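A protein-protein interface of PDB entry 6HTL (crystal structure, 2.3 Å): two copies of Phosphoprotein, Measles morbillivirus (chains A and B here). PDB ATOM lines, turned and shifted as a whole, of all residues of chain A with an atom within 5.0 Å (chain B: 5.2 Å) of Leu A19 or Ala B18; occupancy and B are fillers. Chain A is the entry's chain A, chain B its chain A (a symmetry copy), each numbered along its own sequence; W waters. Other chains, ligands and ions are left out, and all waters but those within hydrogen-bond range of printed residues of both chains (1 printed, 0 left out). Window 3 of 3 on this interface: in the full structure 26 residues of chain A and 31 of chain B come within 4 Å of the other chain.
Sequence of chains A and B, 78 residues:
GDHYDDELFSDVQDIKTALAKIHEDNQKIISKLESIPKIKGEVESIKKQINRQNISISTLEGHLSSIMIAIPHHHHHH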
ATOM      1  N   ILE A  15       7.630 -28.994  30.717  1.00  0.00           N
ATOM      2  CA  ILE A  15       8.724 -29.182  29.768  1.00  0.00           C
ATOM      3  C   ILE A  15      10.003 -28.522  30.292  1.00  0.00           C
ATOM      4  O   ILE A  15      11.067 -29.119  30.199  1.00  0.00           O
ATOM      5  CB  ILE A  15       8.349 -28.728  28.341  1.00  0.00           C
ATOM      6  CG1 ILE A  15       7.288 -29.693  27.718  1.00  0.00           C
ATOM      7  CG2 ILE A  15       9.614 -28.651  27.449  1.00  0.00           C
ATOM      8  CD1 ILE A  15       6.464 -29.052  26.501  1.00  0.00           C
ATOM      9  N   LYS A  16       9.878 -27.318  30.870  1.00  0.00           N
ATOM     10  CA  LYS A  16      10.975 -26.543  31.439  1.00  0.00           C
ATOM     11  C   LYS A  16      11.570 -27.233  32.661  1.00  0.00           C
ATOM     12  O   LYS A  16      12.792 -27.256  32.813  1.00  0.00           O
ATOM     13  CB  LYS A  16      10.495 -25.136  31.784  1.00  0.00           C
ATOM     14  CG  LYS A  16      10.403 -24.241  30.565  1.00  0.00           C
ATOM     15  CD  LYS A  16       9.699 -22.940  30.910  1.00  0.00           C
ATOM     16  CE  LYS A  16      10.160 -21.829  30.018  1.00  0.00           C
ATOM     17  NZ  LYS A  16       9.897 -20.513  30.637  1.00  0.00           N
ATOM     18  N   THR A  17      10.694 -27.819  33.515  1.00  0.00           N
ATOM     19  CA  THR A  17      11.080 -28.554  34.712  1.00  0.00           C
ATOM     20  C   THR A  17      11.859 -29.787  34.302  1.00  0.00           C
ATOM     21  O   THR A  17      12.909 -30.024  34.871  1.00  0.00           O
ATOM     22  CB  THR A  17       9.858 -28.825  35.622  1.00  0.00           C
ATOM     23  OG1 THR A  17       9.328 -27.572  36.053  1.00  0.00           O
ATOM     24  CG2 THR A  17      10.209 -29.662  36.866  1.00  0.00           C
ATOM     25  N   ALA A  18      11.384 -30.527  33.269  1.00  0.00           N
ATOM     26  CA  ALA A  18      12.036 -31.739  32.767  1.00  0.00           C
ATOM     27  C   ALA A  18      13.438 -31.411  32.225  1.00  0.00           C
ATOM     28  O   ALA A  18      14.403 -32.134  32.511  1.00  0.00           O
ATOM     29  CB  ALA A  18      11.183 -32.385  31.687  1.00  0.00           C
ATOM     30  N   LEU A  19      13.541 -30.298  31.461  1.00  0.00           N
ATOM     31  CA  LEU A  19      14.793 -29.810  30.867  1.00  0.00           C
ATOM     32  C   LEU A  19      15.828 -29.467  31.930  1.00  0.00           C
ATOM     33  O   LEU A  19      16.997 -29.797  31.768  1.00  0.00           O
ATOM     34  CB  LEU A  19      14.516 -28.591  29.962  1.00  0.00           C
ATOM     35  CG  LEU A  19      13.788 -28.891  28.645  1.00  0.00           C
ATOM     36  CD1 LEU A  19      13.208 -27.636  28.033  1.00  0.00           C
ATOM     37  CD2 LEU A  19      14.670 -29.648  27.662  1.00  0.00           C
ATOM     38  N   ALA A  20      15.386 -28.803  33.013  1.00  0.00           N
ATOM     39  CA  ALA A  20      16.196 -28.383  34.151  1.00  0.00           C
ATOM     40  C   ALA A  20      16.762 -29.605  34.870  1.00  0.00           C
ATOM     41  O   ALA A  20      17.935 -29.592  35.223  1.00  0.00           O
ATOM     42  CB  ALA A  20      15.361 -27.533  35.103  1.00  0.00           C
ATOM     43  N   LYS A  21      15.957 -30.691  34.998  1.00  0.00           N
ATOM     44  CA  LYS A  21      16.391 -31.938  35.623  1.00  0.00           C
ATOM     45  C   LYS A  21      17.464 -32.649  34.781  1.00  0.00           C
ATOM     46  O   LYS A  21      18.443 -33.106  35.344  1.00  0.00           O
ATOM     47  CB  LYS A  21      15.196 -32.855  35.928  1.00  0.00           C
ATOM     48  N   ILE A  22      17.299 -32.692  33.446  1.00  0.00           N
ATOM     49  CA  ILE A  22      18.248 -33.279  32.502  1.00  0.00           C
ATOM     50  C   ILE A  22      19.591 -32.521  32.547  1.00  0.00           C
ATOM     51  O   ILE A  22      20.648 -33.161  32.571  1.00  0.00           O
ATOM     52  CB  ILE A  22      17.662 -33.337  31.064  1.00  0.00           C
ATOM     53  CG1 ILE A  22      16.456 -34.317  30.988  1.00  0.00           C
ATOM     54  CG2 ILE A  22      18.751 -33.712  30.036  1.00  0.00           C
ATOM     55  CD1 ILE A  22      15.411 -33.963  29.886  1.00  0.00           C
ATOM     56  N   HIS A  23      19.540 -31.166  32.563  1.00  0.00           N
ATOM     57  CA  HIS A  23      20.719 -30.299  32.636  1.00  0.00           C
ATOM     58  C   HIS A  23      21.472 -30.608  33.923  1.00  0.00           C
ATOM     59  O   HIS A  23      22.665 -30.864  33.891  1.00  0.00           O
ATOM     60  CB  HIS A  23      20.295 -28.816  32.590  1.00  0.00           C
ATOM     61  CG  HIS A  23      21.435 -27.861  32.736  1.00  0.00           C
ATOM     62  ND1 HIS A  23      22.228 -27.513  31.653  1.00  0.00           N
ATOM     63  CD2 HIS A  23      21.894 -27.226  33.839  1.00  0.00           C
ATOM     64  CE1 HIS A  23      23.138 -26.678  32.129  1.00  0.00           C
ATOM     65  NE2 HIS A  23      22.984 -26.483  33.444  1.00  0.00           N
ATOM     66  N   GLN B  13      11.466 -20.242  22.929  1.00  0.00           N
ATOM     67  CA  GLN B  13      12.864 -19.859  22.751  1.00  0.00           C
ATOM     68  C   GLN B  13      13.683 -20.331  23.966  1.00  0.00           C
ATOM     69  O   GLN B  13      14.842 -20.693  23.799  1.00  0.00           O
ATOM     70  CB  GLN B  13      12.996 -18.334  22.578  1.00  0.00           C
ATOM     71  CG  GLN B  13      12.302 -17.743  21.349  1.00  0.00           C
ATOM     72  CD  GLN B  13      13.018 -17.970  20.049  1.00  0.00           C
ATOM     73  OE1 GLN B  13      14.057 -17.371  19.776  1.00  0.00           O
ATOM     74  NE2 GLN B  13      12.459 -18.822  19.204  1.00  0.00           N
ATOM     75  N   ASP B  14      13.075 -20.343  25.177  1.00  0.00           N
ATOM     76  CA  ASP B  14      13.698 -20.811  26.423  1.00  0.00           C
ATOM     77  C   ASP B  14      13.934 -22.317  26.315  1.00  0.00           C
ATOM     78  O   ASP B  14      14.972 -22.802  26.753  1.00  0.00           O
ATOM     79  CB  ASP B  14      12.785 -20.543  27.641  1.00  0.00           C
ATOM     80  CG  ASP B  14      12.641 -19.103  28.090  1.00  0.00           C
ATOM     81  OD1 ASP B  14      13.311 -18.211  27.492  1.00  0.00           O
ATOM     82  OD2 ASP B  14      11.868 -18.857  29.039  1.00  0.00           O
ATOM     83  N   ILE B  15      12.940 -23.050  25.749  1.00  0.00           N
ATOM     84  CA  ILE B  15      13.014 -24.493  25.537  1.00  0.00           C
ATOM     85  C   ILE B  15      14.145 -24.832  24.563  1.00  0.00           C
ATOM     86  O   ILE B  15      14.885 -25.776  24.808  1.00  0.00           O
ATOM     87  CB  ILE B  15      11.654 -25.095  25.118  1.00  0.00           C
ATOM     88  CG1 ILE B  15      10.644 -25.052  26.311  1.00  0.00           C
ATOM     89  CG2 ILE B  15      11.841 -26.546  24.607  1.00  0.00           C
ATOM     90  CD1 ILE B  15       9.108 -25.156  25.864  1.00  0.00           C
ATOM     91  N   LYS B  16      14.292 -24.035  23.493  1.00  0.00           N
ATOM     92  CA  LYS B  16      15.317 -24.189  22.467  1.00  0.00           C
ATOM     93  C   LYS B  16      16.712 -23.939  23.031  1.00  0.00           C
ATOM     94  O   LYS B  16      17.643 -24.673  22.698  1.00  0.00           O
ATOM     95  CB  LYS B  16      15.025 -23.257  21.295  1.00  0.00           C
ATOM     96  CG  LYS B  16      13.937 -23.794  20.386  1.00  0.00           C
ATOM     97  CD  LYS B  16      13.512 -22.738  19.382  1.00  0.00           C
ATOM     98  CE  LYS B  16      12.998 -23.369  18.125  1.00  0.00           C
ATOM     99  NZ  LYS B  16      13.064 -22.422  16.993  1.00  0.00           N
ATOM    100  N   THR B  17      16.838 -22.913  23.908  1.00  0.00           N
ATOM    101  CA  THR B  17      18.081 -22.549  24.574  1.00  0.00           C
ATOM    102  C   THR B  17      18.499 -23.684  25.488  1.00  0.00           C
ATOM    103  O   THR B  17      19.652 -24.071  25.440  1.00  0.00           O
ATOM    104  CB  THR B  17      17.966 -21.166  25.259  1.00  0.00           C
ATOM    105  OG1 THR B  17      17.728 -20.182  24.254  1.00  0.00           O
ATOM    106  CG2 THR B  17      19.237 -20.774  26.036  1.00  0.00           C
ATOM    107  N   ALA B  18      17.547 -24.261  26.264  1.00  0.00           N
ATOM    108  CA  ALA B  18      17.810 -25.366  27.189  1.00  0.00           C
ATOM    109  C   ALA B  18      18.303 -26.605  26.421  1.00  0.00           C
ATOM    110  O   ALA B  18      19.271 -27.256  26.841  1.00  0.00           O
ATOM    111  CB  ALA B  18      16.557 -25.694  27.984  1.00  0.00           C
ATOM    112  N   LEU B  19      17.642 -26.906  25.278  1.00  0.00           N
ATOM    113  CA  LEU B  19      17.971 -28.036  24.399  1.00  0.00           C
ATOM    114  C   LEU B  19      19.383 -27.923  23.837  1.00  0.00           C
ATOM    115  O   LEU B  19      20.098 -28.916  23.792  1.00  0.00           O
ATOM    116  CB  LEU B  19      16.937 -28.147  23.260  1.00  0.00           C
ATOM    117  CG  LEU B  19      15.540 -28.631  23.673  1.00  0.00           C
ATOM    118  CD1 LEU B  19      14.510 -28.326  22.609  1.00  0.00           C
ATOM    119  CD2 LEU B  19      15.536 -30.102  24.063  1.00  0.00           C
ATOM    120  N   ALA B  20      19.768 -26.707  23.411  1.00  0.00           N
ATOM    121  CA  ALA B  20      21.071 -26.370  22.847  1.00  0.00           C
ATOM    122  C   ALA B  20      22.164 -26.584  23.891  1.00  0.00           C
ATOM    123  O   ALA B  20      23.203 -27.137  23.553  1.00  0.00           O
ATOM    124  CB  ALA B  20      21.070 -24.927  22.352  1.00  0.00           C
ATOM    125  N   LYS B  21      21.890 -26.234  25.174  1.00  0.00           N
ATOM    126  CA  LYS B  21      22.830 -26.428  26.274  1.00  0.00           C
ATOM    127  C   LYS B  21      23.048 -27.921  26.573  1.00  0.00           C
ATOM    128  O   LYS B  21      24.185 -28.323  26.755  1.00  0.00           O
ATOM    129  CB  LYS B  21      22.396 -25.647  27.525  1.00  0.00           C
ATOM    130  N   ILE B  22      21.975 -28.733  26.572  1.00  0.00           N
ATOM    131  CA  ILE B  22      22.017 -30.179  26.784  1.00  0.00           C
ATOM    132  C   ILE B  22      22.830 -30.864  25.665  1.00  0.00           C
ATOM    133  O   ILE B  22      23.655 -31.734  25.961  1.00  0.00           O
ATOM    134  CB  ILE B  22      20.590 -30.779  26.915  1.00  0.00           C
ATOM    135  CG1 ILE B  22      19.882 -30.268  28.203  1.00  0.00           C
ATOM    136  CG2 ILE B  22      20.631 -32.322  26.877  1.00  0.00           C
ATOM    137  CD1 ILE B  22      18.327 -30.218  28.102  1.00  0.00           C
HETATM  138  O   HOH W   1      19.514 -26.995  29.691  1.00  0.00           O
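NZ of Lys A16 is in salt-bridge range of OD2 of Asp B14 (3.0 Å).
Among the printed residues, pairs that only touch across the chains: Ile A15 with Ile B15 (3.9 Å), Leu A19 with Ile B15 (3.8 Å), Leu A19 with Ala B18 (3.9 Å), Leu A19 with Leu B19 (3.7 Å), Leu A19 with Ile B22 (3.7 Å) and Ile A22 with Ile B22 (3.9 Å).
Printed residues of chain B within 4 Å of Lys A16: Asp B14. Of chain B, only Ile B15 (3.8 Å), Ala B18 (3.9 Å), Leu B19 (3.7 Å) and Ile B22 (3.7 Å) come within 4 Å of Leu A19. Of the printed residues of chain A, Ile B15 touches Ile A15 and Leu A19. Of the printed residues of chain A, Ala B18 touches Leu A19. Lys B21 touches none of the printed residues of chain A. Of the printed residues of chain A, Ile B22 touches Leu A19 (3.7 Å) and Ile A22 (3.9 Å). The nearest printed residue of chain B that does not touch Leu A19 is Asp B14 (5.3 Å). The nearest printed residue of chain A that does not touch Ala B18 is His A23 (5.7 Å).
Among the printed residues, 7 pairs touch across the chains.
Ile B15 touches its own counterpart, Ile A15. Leu A19 touches Ile B15, but with the chains exchanged Ile A15 does not touch Leu B19 (6.9 Å). Leu B19 touches its own counterpart, Leu A19. Leu A19 touches Ile B22, but with the chains exchanged Ile A22 does not touch Leu B19 (7.0 Å). Positions printed for both chains: 15, 16, 17, 18, 19, 20, 21 and 22. Of the 7 pairs that touch across the chains among the printed residues, 3 have their exchanged pair printed and touching as well.
Water W1 lies within hydrogen-bond range of O of Ala B18 and ND1 of His A23.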
